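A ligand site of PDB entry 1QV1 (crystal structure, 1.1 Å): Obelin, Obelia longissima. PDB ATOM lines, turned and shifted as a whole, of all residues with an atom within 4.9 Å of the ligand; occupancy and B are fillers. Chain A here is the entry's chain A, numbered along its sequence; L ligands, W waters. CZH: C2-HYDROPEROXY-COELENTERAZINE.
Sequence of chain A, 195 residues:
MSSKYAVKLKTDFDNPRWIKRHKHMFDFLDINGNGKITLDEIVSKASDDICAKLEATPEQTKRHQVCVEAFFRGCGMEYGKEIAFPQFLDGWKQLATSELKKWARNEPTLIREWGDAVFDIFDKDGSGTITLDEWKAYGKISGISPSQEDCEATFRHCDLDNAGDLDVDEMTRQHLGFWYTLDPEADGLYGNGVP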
ATOM      1  N   HIS A  22      14.268  28.170  23.178  1.00  0.00           N
ATOM      2  CA  HIS A  22      12.895  28.389  22.706  1.00  0.00           C
ATOM      3  C   HIS A  22      12.836  29.112  21.409  1.00  0.00           C
ATOM      4  O   HIS A  22      11.879  28.884  20.651  1.00  0.00           O
ATOM      5  CB  HIS A  22      12.098  29.108  23.839  1.00  0.00           C
ATOM      6  CG  HIS A  22      11.804  28.144  24.923  1.00  0.00           C
ATOM      7  ND1 HIS A  22      10.901  27.129  24.748  1.00  0.00           N
ATOM      8  CD2 HIS A  22      12.339  28.064  26.159  1.00  0.00           C
ATOM      9  CE1 HIS A  22      10.888  26.449  25.874  1.00  0.00           C
ATOM     10  NE2 HIS A  22      11.737  26.979  26.741  1.00  0.00           N
ATOM     11  N   MET A  25      13.081  26.495  18.877  1.00  0.00           N
ATOM     12  CA  MET A  25      11.807  25.747  18.723  1.00  0.00           C
ATOM     13  C   MET A  25      10.752  26.578  18.047  1.00  0.00           C
ATOM     14  O   MET A  25      10.020  26.056  17.211  1.00  0.00           O
ATOM     15  CB  MET A  25      11.330  25.294  20.099  1.00  0.00           C
ATOM     16  CG  MET A  25      12.206  24.221  20.723  1.00  0.00           C
ATOM     17  SD  MET A  25      12.537  22.770  19.725  1.00  0.00           S
ATOM     18  CE  MET A  25      10.860  22.189  19.447  1.00  0.00           C
ATOM     19  N   PHE A  26      10.640  27.868  18.392  1.00  0.00           N
ATOM     20  CA  PHE A  26       9.657  28.711  17.734  1.00  0.00           C
ATOM     21  C   PHE A  26       9.936  28.706  16.248  1.00  0.00           C
ATOM     22  O   PHE A  26       9.015  28.596  15.438  1.00  0.00           O
ATOM     23  CB  PHE A  26       9.772  30.123  18.348  1.00  0.00           C
ATOM     24  CG  PHE A  26       8.763  31.067  17.714  1.00  0.00           C
ATOM     25  CD1 PHE A  26       7.524  31.262  18.324  1.00  0.00           C
ATOM     26  CD2 PHE A  26       9.032  31.770  16.542  1.00  0.00           C
ATOM     27  CE1 PHE A  26       6.581  32.105  17.760  1.00  0.00           C
ATOM     28  CE2 PHE A  26       8.098  32.560  15.961  1.00  0.00           C
ATOM     29  CZ  PHE A  26       6.873  32.769  16.580  1.00  0.00           C
ATOM     30  N   PHE A  28      11.446  26.629  14.435  1.00  0.00           N
ATOM     31  CA  PHE A  28      11.100  25.300  13.926  1.00  0.00           C
ATOM     32  C   PHE A  28       9.614  25.156  13.700  1.00  0.00           C
ATOM     33  O   PHE A  28       9.191  24.523  12.718  1.00  0.00           O
ATOM     34  CB  PHE A  28      11.649  24.283  14.912  1.00  0.00           C
ATOM     35  CG  PHE A  28      10.975  22.895  14.938  1.00  0.00           C
ATOM     36  CD1 PHE A  28      11.232  21.914  14.031  1.00  0.00           C
ATOM     37  CD2 PHE A  28      10.070  22.654  15.956  1.00  0.00           C
ATOM     38  CE1 PHE A  28      10.599  20.681  14.133  1.00  0.00           C
ATOM     39  CE2 PHE A  28       9.467  21.403  16.131  1.00  0.00           C
ATOM     40  CZ  PHE A  28       9.735  20.390  15.189  1.00  0.00           C
ATOM     41  N   LEU A  29       8.794  25.728  14.573  1.00  0.00           N
ATOM     42  CA  LEU A  29       7.321  25.696  14.380  1.00  0.00           C
ATOM     43  C   LEU A  29       6.880  26.689  13.332  1.00  0.00           C
ATOM     44  O   LEU A  29       5.838  26.423  12.701  1.00  0.00           O
ATOM     45  CB  LEU A  29       6.649  25.979  15.698  1.00  0.00           C
ATOM     46  CG  LEU A  29       6.872  24.891  16.758  1.00  0.00           C
ATOM     47  CD1 LEU A  29       6.324  25.356  18.081  1.00  0.00           C
ATOM     48  CD2 LEU A  29       6.226  23.593  16.316  1.00  0.00           C
ATOM     49  N   ILE A  42      -0.104  24.082  15.779  1.00  0.00           N
ATOM     50  CA  ILE A  42       0.506  23.156  16.695  1.00  0.00           C
ATOM     51  C   ILE A  42      -0.346  21.899  16.817  1.00  0.00           C
ATOM     52  O   ILE A  42       0.139  20.780  16.825  1.00  0.00           O
ATOM     53  CB  ILE A  42       0.761  23.860  18.042  1.00  0.00           C
ATOM     54  CG1 ILE A  42       2.052  24.684  17.908  1.00  0.00           C
ATOM     55  CG2 ILE A  42       0.833  22.861  19.176  1.00  0.00           C
ATOM     56  CD1 ILE A  42       2.161  25.506  19.167  1.00  0.00           C
ATOM     57  N   LYS A  45      -0.124  19.773  13.728  1.00  0.00           N
ATOM     58  CA  LYS A  45       1.128  19.023  13.708  1.00  0.00           C
ATOM     59  C   LYS A  45       0.979  17.829  14.641  1.00  0.00           C
ATOM     60  O   LYS A  45       1.369  16.728  14.304  1.00  0.00           O
ATOM     61  CB  LYS A  45       2.228  19.953  14.202  1.00  0.00           C
ATOM     62  CG  LYS A  45       3.594  19.299  14.314  1.00  0.00           C
ATOM     63  CD  LYS A  45       4.650  20.339  14.721  1.00  0.00           C
ATOM     64  CE  LYS A  45       6.049  19.761  14.871  1.00  0.00           C
ATOM     65  NZ  LYS A  45       6.615  19.380  13.550  1.00  0.00           N
ATOM     66  N   ALA A  46       0.452  18.014  15.840  1.00  0.00           N
ATOM     67  CA  ALA A  46       0.271  16.924  16.758  1.00  0.00           C
ATOM     68  C   ALA A  46      -0.625  15.824  16.236  1.00  0.00           C
ATOM     69  O   ALA A  46      -0.310  14.650  16.313  1.00  0.00           O
ATOM     70  CB  ALA A  46      -0.316  17.462  18.070  1.00  0.00           C
ATOM     71  N   ILE A  50       1.857  14.026  13.340  1.00  0.00           N
ATOM     72  CA  ILE A  50       2.528  13.095  14.252  1.00  0.00           C
ATOM     73  C   ILE A  50       1.684  11.887  14.582  1.00  0.00           C
ATOM     74  O   ILE A  50       2.102  10.759  14.417  1.00  0.00           O
ATOM     75  CB  ILE A  50       2.973  13.840  15.508  1.00  0.00           C
ATOM     76  CG1 ILE A  50       4.079  14.852  15.141  1.00  0.00           C
ATOM     77  CG2 ILE A  50       3.484  12.874  16.577  1.00  0.00           C
ATOM     78  CD1 ILE A  50       4.418  15.865  16.230  1.00  0.00           C
ATOM     79  N   VAL A  68      -1.727  18.379  24.313  1.00  0.00           N
ATOM     80  CA  VAL A  68      -1.031  19.434  23.539  1.00  0.00           C
ATOM     81  C   VAL A  68      -1.761  20.754  23.683  1.00  0.00           C
ATOM     82  O   VAL A  68      -1.133  21.806  23.871  1.00  0.00           O
ATOM     83  CB  VAL A  68      -0.878  18.950  22.087  1.00  0.00           C
ATOM     84  CG1 VAL A  68      -0.491  20.133  21.208  1.00  0.00           C
ATOM     85  CG2 VAL A  68       0.116  17.829  22.006  1.00  0.00           C
ATOM     86  N   PHE A  72       0.123  23.975  25.386  1.00  0.00           N
ATOM     87  CA  PHE A  72       0.389  25.205  24.658  1.00  0.00           C
ATOM     88  C   PHE A  72      -0.546  26.308  25.066  1.00  0.00           C
ATOM     89  O   PHE A  72      -0.148  27.494  25.050  1.00  0.00           O
ATOM     90  CB  PHE A  72       0.417  24.969  23.142  1.00  0.00           C
ATOM     91  CG  PHE A  72       1.745  24.281  22.794  1.00  0.00           C
ATOM     92  CD1 PHE A  72       1.758  22.892  22.600  1.00  0.00           C
ATOM     93  CD2 PHE A  72       2.919  25.016  22.698  1.00  0.00           C
ATOM     94  CE1 PHE A  72       2.975  22.254  22.322  1.00  0.00           C
ATOM     95  CE2 PHE A  72       4.137  24.364  22.394  1.00  0.00           C
ATOM     96  CZ  PHE A  72       4.151  22.987  22.235  1.00  0.00           C
ATOM     97  N   PHE A  88       5.364  34.494  22.920  1.00  0.00           N
ATOM     98  CA  PHE A  88       5.500  33.059  23.129  1.00  0.00           C
ATOM     99  C   PHE A  88       6.437  32.784  24.292  1.00  0.00           C
ATOM    100  O   PHE A  88       6.147  31.968  25.167  1.00  0.00           O
ATOM    101  CB  PHE A  88       6.034  32.484  21.840  1.00  0.00           C
ATOM    102  CG  PHE A  88       6.204  30.996  21.800  1.00  0.00           C
ATOM    103  CD1 PHE A  88       5.113  30.154  21.702  1.00  0.00           C
ATOM    104  CD2 PHE A  88       7.493  30.474  21.810  1.00  0.00           C
ATOM    105  CE1 PHE A  88       5.311  28.789  21.569  1.00  0.00           C
ATOM    106  CE2 PHE A  88       7.698  29.103  21.651  1.00  0.00           C
ATOM    107  CZ  PHE A  88       6.603  28.287  21.538  1.00  0.00           C
ATOM    108  N   TRP A  92       5.987  30.935  27.913  1.00  0.00           N
ATOM    109  CA  TRP A  92       6.791  29.873  28.514  1.00  0.00           C
ATOM    110  C   TRP A  92       7.239  30.212  29.901  1.00  0.00           C
ATOM    111  O   TRP A  92       7.347  29.326  30.736  1.00  0.00           O
ATOM    112  CB  TRP A  92       8.027  29.603  27.641  1.00  0.00           C
ATOM    113  CG  TRP A  92       7.713  28.620  26.561  1.00  0.00           C
ATOM    114  CD1 TRP A  92       7.285  28.869  25.312  1.00  0.00           C
ATOM    115  CD2 TRP A  92       7.790  27.198  26.721  1.00  0.00           C
ATOM    116  NE1 TRP A  92       7.108  27.664  24.653  1.00  0.00           N
ATOM    117  CE2 TRP A  92       7.405  26.642  25.487  1.00  0.00           C
ATOM    118  CE3 TRP A  92       8.156  26.351  27.747  1.00  0.00           C
ATOM    119  CZ2 TRP A  92       7.361  25.290  25.269  1.00  0.00           C
ATOM    120  CZ3 TRP A  92       8.127  24.988  27.521  1.00  0.00           C
ATOM    121  CH2 TRP A  92       7.745  24.478  26.286  1.00  0.00           C
ATOM    122  N   ILE A 111       3.737  18.919  31.237  1.00  0.00           N
ATOM    123  CA  ILE A 111       4.766  18.236  30.460  1.00  0.00           C
ATOM    124  C   ILE A 111       4.749  16.749  30.787  1.00  0.00           C
ATOM    125  O   ILE A 111       4.984  15.913  29.881  1.00  0.00           O
ATOM    126  CB  ILE A 111       6.149  18.889  30.634  1.00  0.00           C
ATOM    127  CG1 ILE A 111       7.165  18.329  29.626  1.00  0.00           C
ATOM    128  CG2 ILE A 111       6.675  18.760  32.072  1.00  0.00           C
ATOM    129  CD1 ILE A 111       6.796  18.462  28.178  1.00  0.00           C
ATOM    130  N   TRP A 114       1.664  15.360  28.795  1.00  0.00           N
ATOM    131  CA  TRP A 114       1.982  15.235  27.375  1.00  0.00           C
ATOM    132  C   TRP A 114       2.871  14.001  27.175  1.00  0.00           C
ATOM    133  O   TRP A 114       2.608  13.206  26.287  1.00  0.00           O
ATOM    134  CB  TRP A 114       2.612  16.521  26.909  1.00  0.00           C
ATOM    135  CG  TRP A 114       2.848  16.555  25.418  1.00  0.00           C
ATOM    136  CD1 TRP A 114       2.394  15.704  24.451  1.00  0.00           C
ATOM    137  CD2 TRP A 114       3.612  17.568  24.739  1.00  0.00           C
ATOM    138  NE1 TRP A 114       2.820  16.075  23.220  1.00  0.00           N
ATOM    139  CE2 TRP A 114       3.568  17.226  23.360  1.00  0.00           C
ATOM    140  CE3 TRP A 114       4.310  18.699  25.140  1.00  0.00           C
ATOM    141  CZ2 TRP A 114       4.199  17.997  22.410  1.00  0.00           C
ATOM    142  CZ3 TRP A 114       4.959  19.481  24.184  1.00  0.00           C
ATOM    143  CH2 TRP A 114       4.894  19.107  22.829  1.00  0.00           C
ATOM    144  N   GLY A 115       3.880  13.863  28.009  1.00  0.00           N
ATOM    145  CA  GLY A 115       4.700  12.689  27.920  1.00  0.00           C
ATOM    146  C   GLY A 115       3.884  11.397  28.029  1.00  0.00           C
ATOM    147  O   GLY A 115       4.100  10.446  27.291  1.00  0.00           O
ATOM    148  N   VAL A 118       2.341  10.686  24.738  1.00  0.00           N
ATOM    149  CA  VAL A 118       3.289  10.265  23.704  1.00  0.00           C
ATOM    150  C   VAL A 118       3.722   8.852  23.984  1.00  0.00           C
ATOM    151  O   VAL A 118       3.720   7.981  23.102  1.00  0.00           O
ATOM    152  CB  VAL A 118       4.480  11.217  23.666  1.00  0.00           C
ATOM    153  CG1 VAL A 118       5.561  10.651  22.707  1.00  0.00           C
ATOM    154  CG2 VAL A 118       4.090  12.611  23.230  1.00  0.00           C
ATOM    155  N   PHE A 119       4.103   8.587  25.260  1.00  0.00           N
ATOM    156  CA  PHE A 119       4.548   7.250  25.587  1.00  0.00           C
ATOM    157  C   PHE A 119       3.455   6.238  25.336  1.00  0.00           C
ATOM    158  O   PHE A 119       3.767   5.114  24.893  1.00  0.00           O
ATOM    159  CB  PHE A 119       4.998   7.160  27.056  1.00  0.00           C
ATOM    160  CG  PHE A 119       6.392   7.652  27.296  1.00  0.00           C
ATOM    161  CD1 PHE A 119       6.790   8.965  27.112  1.00  0.00           C
ATOM    162  CD2 PHE A 119       7.331   6.713  27.760  1.00  0.00           C
ATOM    163  CE1 PHE A 119       8.103   9.318  27.374  1.00  0.00           C
ATOM    164  CE2 PHE A 119       8.650   7.097  27.972  1.00  0.00           C
ATOM    165  CZ  PHE A 119       9.040   8.415  27.792  1.00  0.00           C
ATOM    166  N   TRP A 135      12.102   6.351  19.941  1.00  0.00           N
ATOM    167  CA  TRP A 135      12.543   7.752  20.072  1.00  0.00           C
ATOM    168  C   TRP A 135      13.086   8.258  18.725  1.00  0.00           C
ATOM    169  O   TRP A 135      12.810   9.387  18.354  1.00  0.00           O
ATOM    170  CB  TRP A 135      13.537   7.905  21.184  1.00  0.00           C
ATOM    171  CG  TRP A 135      13.879   9.315  21.458  1.00  0.00           C
ATOM    172  CD1 TRP A 135      15.159   9.814  21.403  1.00  0.00           C
ATOM    173  CD2 TRP A 135      13.041  10.377  21.850  1.00  0.00           C
ATOM    174  NE1 TRP A 135      15.166  11.145  21.720  1.00  0.00           N
ATOM    175  CE2 TRP A 135      13.865  11.514  21.977  1.00  0.00           C
ATOM    176  CE3 TRP A 135      11.675  10.501  22.073  1.00  0.00           C
ATOM    177  CZ2 TRP A 135      13.362  12.762  22.342  1.00  0.00           C
ATOM    178  CZ3 TRP A 135      11.189  11.750  22.419  1.00  0.00           C
ATOM    179  CH2 TRP A 135      12.040  12.846  22.548  1.00  0.00           C
ATOM    180  N   TYR A 138      10.148   9.115  16.652  1.00  0.00           N
ATOM    181  CA  TYR A 138       9.538  10.341  17.111  1.00  0.00           C
ATOM    182  C   TYR A 138      10.372  11.528  16.647  1.00  0.00           C
ATOM    183  O   TYR A 138       9.838  12.549  16.189  1.00  0.00           O
ATOM    184  CB  TYR A 138       9.364  10.303  18.664  1.00  0.00           C
ATOM    185  CG  TYR A 138       8.658  11.601  19.037  1.00  0.00           C
ATOM    186  CD1 TYR A 138       7.305  11.718  18.853  1.00  0.00           C
ATOM    187  CD2 TYR A 138       9.353  12.736  19.518  1.00  0.00           C
ATOM    188  CE1 TYR A 138       6.623  12.879  19.148  1.00  0.00           C
ATOM    189  CE2 TYR A 138       8.676  13.905  19.790  1.00  0.00           C
ATOM    190  CZ  TYR A 138       7.301  13.989  19.630  1.00  0.00           C
ATOM    191  OH  TYR A 138       6.621  15.135  19.854  1.00  0.00           O
ATOM    192  N   SER A 142       8.150  13.983  14.493  1.00  0.00           N
ATOM    193  CA  SER A 142       7.899  15.334  15.033  1.00  0.00           C
ATOM    194  C   SER A 142       8.822  16.352  14.412  1.00  0.00           C
ATOM    195  O   SER A 142       8.514  17.524  14.464  1.00  0.00           O
ATOM    196  CB  SER A 142       8.107  15.332  16.536  1.00  0.00           C
ATOM    197  OG  SER A 142       9.494  15.268  16.853  1.00  0.00           O
ATOM    198  N   ILE A 144      11.650  17.137  15.694  1.00  0.00           N
ATOM    199  CA  ILE A 144      12.519  17.824  16.669  1.00  0.00           C
ATOM    200  C   ILE A 144      13.919  17.300  16.643  1.00  0.00           C
ATOM    201  O   ILE A 144      14.854  18.025  17.044  1.00  0.00           O
ATOM    202  CB  ILE A 144      11.888  17.699  18.069  1.00  0.00           C
ATOM    203  CG1 ILE A 144      12.481  18.722  19.009  1.00  0.00           C
ATOM    204  CG2 ILE A 144      11.944  16.278  18.649  1.00  0.00           C
ATOM    205  CD1 ILE A 144      11.662  18.837  20.291  1.00  0.00           C
ATOM    206  N   VAL A 168       9.109   7.551  31.284  1.00  0.00           N
ATOM    207  CA  VAL A 168       8.469   8.867  31.267  1.00  0.00           C
ATOM    208  C   VAL A 168       8.811   9.643  32.518  1.00  0.00           C
ATOM    209  O   VAL A 168       8.877  10.878  32.474  1.00  0.00           O
ATOM    210  CB  VAL A 168       6.962   8.750  31.067  1.00  0.00           C
ATOM    211  CG1 VAL A 168       6.306   8.134  32.277  1.00  0.00           C
ATOM    212  CG2 VAL A 168       6.360  10.117  30.735  1.00  0.00           C
ATOM    213  N   MET A 171      12.158  11.108  31.595  1.00  0.00           N
ATOM    214  CA  MET A 171      12.053  12.132  30.537  1.00  0.00           C
ATOM    215  C   MET A 171      11.368  13.384  31.067  1.00  0.00           C
ATOM    216  O   MET A 171      11.662  14.507  30.623  1.00  0.00           O
ATOM    217  CB  MET A 171      11.324  11.573  29.313  1.00  0.00           C
ATOM    218  CG  MET A 171      11.470  12.488  28.100  1.00  0.00           C
ATOM    219  SD  MET A 171      13.210  12.808  27.709  1.00  0.00           S
ATOM    220  CE  MET A 171      13.106  13.094  25.944  1.00  0.00           C
ATOM    221  N   THR A 172      10.449  13.233  32.003  1.00  0.00           N
ATOM    222  CA  THR A 172       9.779  14.393  32.571  1.00  0.00           C
ATOM    223  C   THR A 172      10.763  15.203  33.395  1.00  0.00           C
ATOM    224  O   THR A 172      10.817  16.434  33.311  1.00  0.00           O
ATOM    225  CB  THR A 172       8.593  13.948  33.434  1.00  0.00           C
ATOM    226  OG1 THR A 172       7.637  13.321  32.587  1.00  0.00           O
ATOM    227  CG2 THR A 172       7.952  15.163  34.081  1.00  0.00           C
ATOM    228  N   HIS A 175      12.868  16.990  30.959  1.00  0.00           N
ATOM    229  CA  HIS A 175      12.138  18.075  30.321  1.00  0.00           C
ATOM    230  C   HIS A 175      11.896  19.250  31.237  1.00  0.00           C
ATOM    231  O   HIS A 175      11.907  20.390  30.748  1.00  0.00           O
ATOM    232  CB  HIS A 175      10.806  17.548  29.790  1.00  0.00           C
ATOM    233  CG  HIS A 175      10.939  16.947  28.440  1.00  0.00           C
ATOM    234  ND1 HIS A 175       9.983  16.090  27.926  1.00  0.00           N
ATOM    235  CD2 HIS A 175      11.817  17.171  27.440  1.00  0.00           C
ATOM    236  CE1 HIS A 175      10.341  15.776  26.676  1.00  0.00           C
ATOM    237  NE2 HIS A 175      11.455  16.424  26.327  1.00  0.00           N
ATOM    238  N   TRP A 179      13.283  22.370  29.320  1.00  0.00           N
ATOM    239  CA  TRP A 179      12.399  23.392  28.831  1.00  0.00           C
ATOM    240  C   TRP A 179      12.144  24.518  29.829  1.00  0.00           C
ATOM    241  O   TRP A 179      11.912  25.640  29.404  1.00  0.00           O
ATOM    242  CB  TRP A 179      11.046  22.821  28.409  1.00  0.00           C
ATOM    243  CG  TRP A 179      11.097  21.815  27.315  1.00  0.00           C
ATOM    244  CD1 TRP A 179      10.488  20.577  27.373  1.00  0.00           C
ATOM    245  CD2 TRP A 179      11.716  21.915  26.037  1.00  0.00           C
ATOM    246  NE1 TRP A 179      10.710  19.912  26.226  1.00  0.00           N
ATOM    247  CE2 TRP A 179      11.449  20.685  25.365  1.00  0.00           C
ATOM    248  CE3 TRP A 179      12.443  22.904  25.367  1.00  0.00           C
ATOM    249  CZ2 TRP A 179      11.902  20.404  24.105  1.00  0.00           C
ATOM    250  CZ3 TRP A 179      12.893  22.625  24.098  1.00  0.00           C
ATOM    251  CH2 TRP A 179      12.619  21.377  23.480  1.00  0.00           C
ATOM    252  N   TYR A 190      18.652  16.530  23.726  1.00  0.00           N
ATOM    253  CA  TYR A 190      18.303  16.245  22.355  1.00  0.00           C
ATOM    254  C   TYR A 190      19.575  16.226  21.508  1.00  0.00           C
ATOM    255  O   TYR A 190      19.553  16.510  20.320  1.00  0.00           O
ATOM    256  CB  TYR A 190      17.338  17.306  21.799  1.00  0.00           C
ATOM    257  CG  TYR A 190      15.939  17.150  22.378  1.00  0.00           C
ATOM    258  CD1 TYR A 190      15.553  17.673  23.592  1.00  0.00           C
ATOM    259  CD2 TYR A 190      14.990  16.414  21.668  1.00  0.00           C
ATOM    260  CE1 TYR A 190      14.278  17.517  24.085  1.00  0.00           C
ATOM    261  CE2 TYR A 190      13.717  16.244  22.136  1.00  0.00           C
ATOM    262  CZ  TYR A 190      13.371  16.778  23.358  1.00  0.00           C
ATOM    263  OH  TYR A 190      12.094  16.561  23.782  1.00  0.00           O
HETATM  264  N1  CZH L   1       7.838  16.985  21.439  1.00  0.00           N
HETATM  265  C2  CZH L   1       8.132  16.465  22.700  1.00  0.00           C
HETATM  266  C3  CZH L   1       8.507  17.701  23.573  1.00  0.00           C
HETATM  267  N4  CZH L   1       8.307  18.732  22.756  1.00  0.00           N
HETATM  268  C5  CZH L   1       8.505  20.117  23.062  1.00  0.00           C
HETATM  269  C6  CZH L   1       8.341  21.012  22.030  1.00  0.00           C
HETATM  270  N7  CZH L   1       7.962  20.545  20.726  1.00  0.00           N
HETATM  271  C8  CZH L   1       7.799  19.271  20.489  1.00  0.00           C
HETATM  272  C9  CZH L   1       7.951  18.276  21.524  1.00  0.00           C
HETATM  273  C10 CZH L   1       6.948  15.568  23.216  1.00  0.00           C
HETATM  274  C11 CZH L   1       7.218  14.897  24.493  1.00  0.00           C
HETATM  275  C12 CZH L   1       7.954  13.638  24.518  1.00  0.00           C
HETATM  276  C13 CZH L   1       8.238  12.955  25.697  1.00  0.00           C
HETATM  277  C14 CZH L   1       7.779  13.563  26.940  1.00  0.00           C
HETATM  278  C15 CZH L   1       7.063  14.787  26.943  1.00  0.00           C
HETATM  279  C16 CZH L   1       6.789  15.460  25.701  1.00  0.00           C
HETATM  280  O17 CZH L   1       8.117  12.951  28.059  1.00  0.00           O
HETATM  281  O18 CZH L   1       8.850  17.768  24.724  1.00  0.00           O
HETATM  282  C19 CZH L   1       8.557  22.406  22.197  1.00  0.00           C
HETATM  283  C20 CZH L   1       7.910  23.334  21.352  1.00  0.00           C
HETATM  284  C21 CZH L   1       8.169  24.711  21.497  1.00  0.00           C
HETATM  285  C22 CZH L   1       9.097  25.169  22.491  1.00  0.00           C
HETATM  286  C23 CZH L   1       9.747  24.237  23.300  1.00  0.00           C
HETATM  287  C24 CZH L   1       9.458  22.880  23.194  1.00  0.00           C
HETATM  288  O25 CZH L   1       9.328  26.479  22.575  1.00  0.00           O
HETATM  289  C26 CZH L   1       7.410  18.844  19.100  1.00  0.00           C
HETATM  290  C27 CZH L   1       5.958  19.168  18.853  1.00  0.00           C
HETATM  291  C28 CZH L   1       5.013  18.125  18.800  1.00  0.00           C
HETATM  292  C29 CZH L   1       3.620  18.410  18.563  1.00  0.00           C
HETATM  293  C30 CZH L   1       3.241  19.754  18.388  1.00  0.00           C
HETATM  294  C31 CZH L   1       4.185  20.836  18.463  1.00  0.00           C
HETATM  295  C32 CZH L   1       5.546  20.511  18.714  1.00  0.00           C
HETATM  296  O33 CZH L   1       9.256  15.535  22.622  1.00  0.00           O
HETATM  297  O34 CZH L   1      10.270  16.300  21.966  1.00  0.00           O
HETATM  298  O   HOH W   1       3.825  15.235  19.901  1.00  0.00           O
HETATM  299  O   HOH W   2       7.432  14.506  30.143  1.00  0.00           O
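The side-chain hydroxyl (OH) of Tyr 190 sits at hydrogen-bond distance from a ring nitrogen (NE2) of His 175, at 2.6 Å.
A ring nitrogen (NE2) of His 22 lies within hydrogen-bond range of the backbone carbonyl oxygen (O) of Trp 179, 3.0 Å away.
The side-chain hydroxyl of Ser 142 lies within hydrogen-bond range of the backbone NH of Ile 144 (3.1 Å).
O of Tyr 138 sits at hydrogen-bond distance from OG of Ser 142, 2.8 Å away.
The side-chain amino group (NZ) of Lys 45 lies within hydrogen-bond range of the backbone carbonyl oxygen (O) of Ser 142 (2.8 Å).
The backbone NH of Ile 50 is in hydrogen-bond range of the backbone carbonyl oxygen of Lys 45, at 2.9 Å.
Water W2 lies within hydrogen-bond range of O17 of the ligand, OG1 of Thr 172 and O of Ile 111.
Met 25 touches the ligand.
Leu 29 touches the ligand (CD1 to C21, 3.9 Å).
Ile 42 touches the ligand (O to C30, 3.6 Å).
CD of Lys 45 touches C31 of the ligand, 3.8 Å away.
Ile 50 touches the ligand.
Phe 72 touches the ligand (CZ to C20, 3.9 Å).
Phe 88 touches the ligand (CE2 to O25, 3.2 Å).
Ile 111 touches the ligand.
Trp 114 touches the ligand (CH2 to C9, 3.4 Å).
Gly 115 touches the ligand (CA to C15, 3.3 Å).
Phe 119 touches the ligand (CE1 to O17, 3.7 Å).
Trp 135 touches the ligand (CH2 to O33, 3.9 Å).
Ile 144 touches the ligand.
CG of Met 171 touches O17 of the ligand (3.4 Å).
Hydrophobic or aromatic side chains within 4 Å of the ligand: His 22, Met 25, Leu 29, Ile 42, Ile 50, Phe 72, Phe 88, Trp 92, Ile 111, Trp 114, Phe 119, Trp 135, Tyr 138, Ile 144, Met 171, His 175, Trp 179 and Tyr 190.
Within 4 Å of the ligand: His 22, Met 25, Leu 29, Ile 42, Lys 45, Ile 50, Phe 72, Phe 88, Trp 92, Ile 111, Trp 114, Gly 115, Phe 119, Trp 135, Tyr 138, Ile 144, Met 171, His 175, Trp 179 and Tyr 190.
Along chain A the residues within 4 Å of the ligand span positions 22 to 190.
O18 of the ligand sits at hydrogen-bond distance from NE1 of Trp 179 (3.2 Å).
OH of Tyr 190 lies within hydrogen-bond range of O34 of the ligand, 2.6 Å away.
The indole nitrogen (NE1) of Trp 92 sits at hydrogen-bond distance from an oxygen (O25) of the ligand, at 3.3 Å.
A nitrogen (N1) of the ligand sits at hydrogen-bond distance from the side-chain hydroxyl (OH) of Tyr 138 (2.7 Å).
A ring nitrogen (ND1) of His 22 lies within hydrogen-bond range of an oxygen (O25) of the ligand, at 2.8 Å.
An oxygen (O18) of the ligand sits close to a ring nitrogen (NE2) of His 175, at 3.3 Å.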
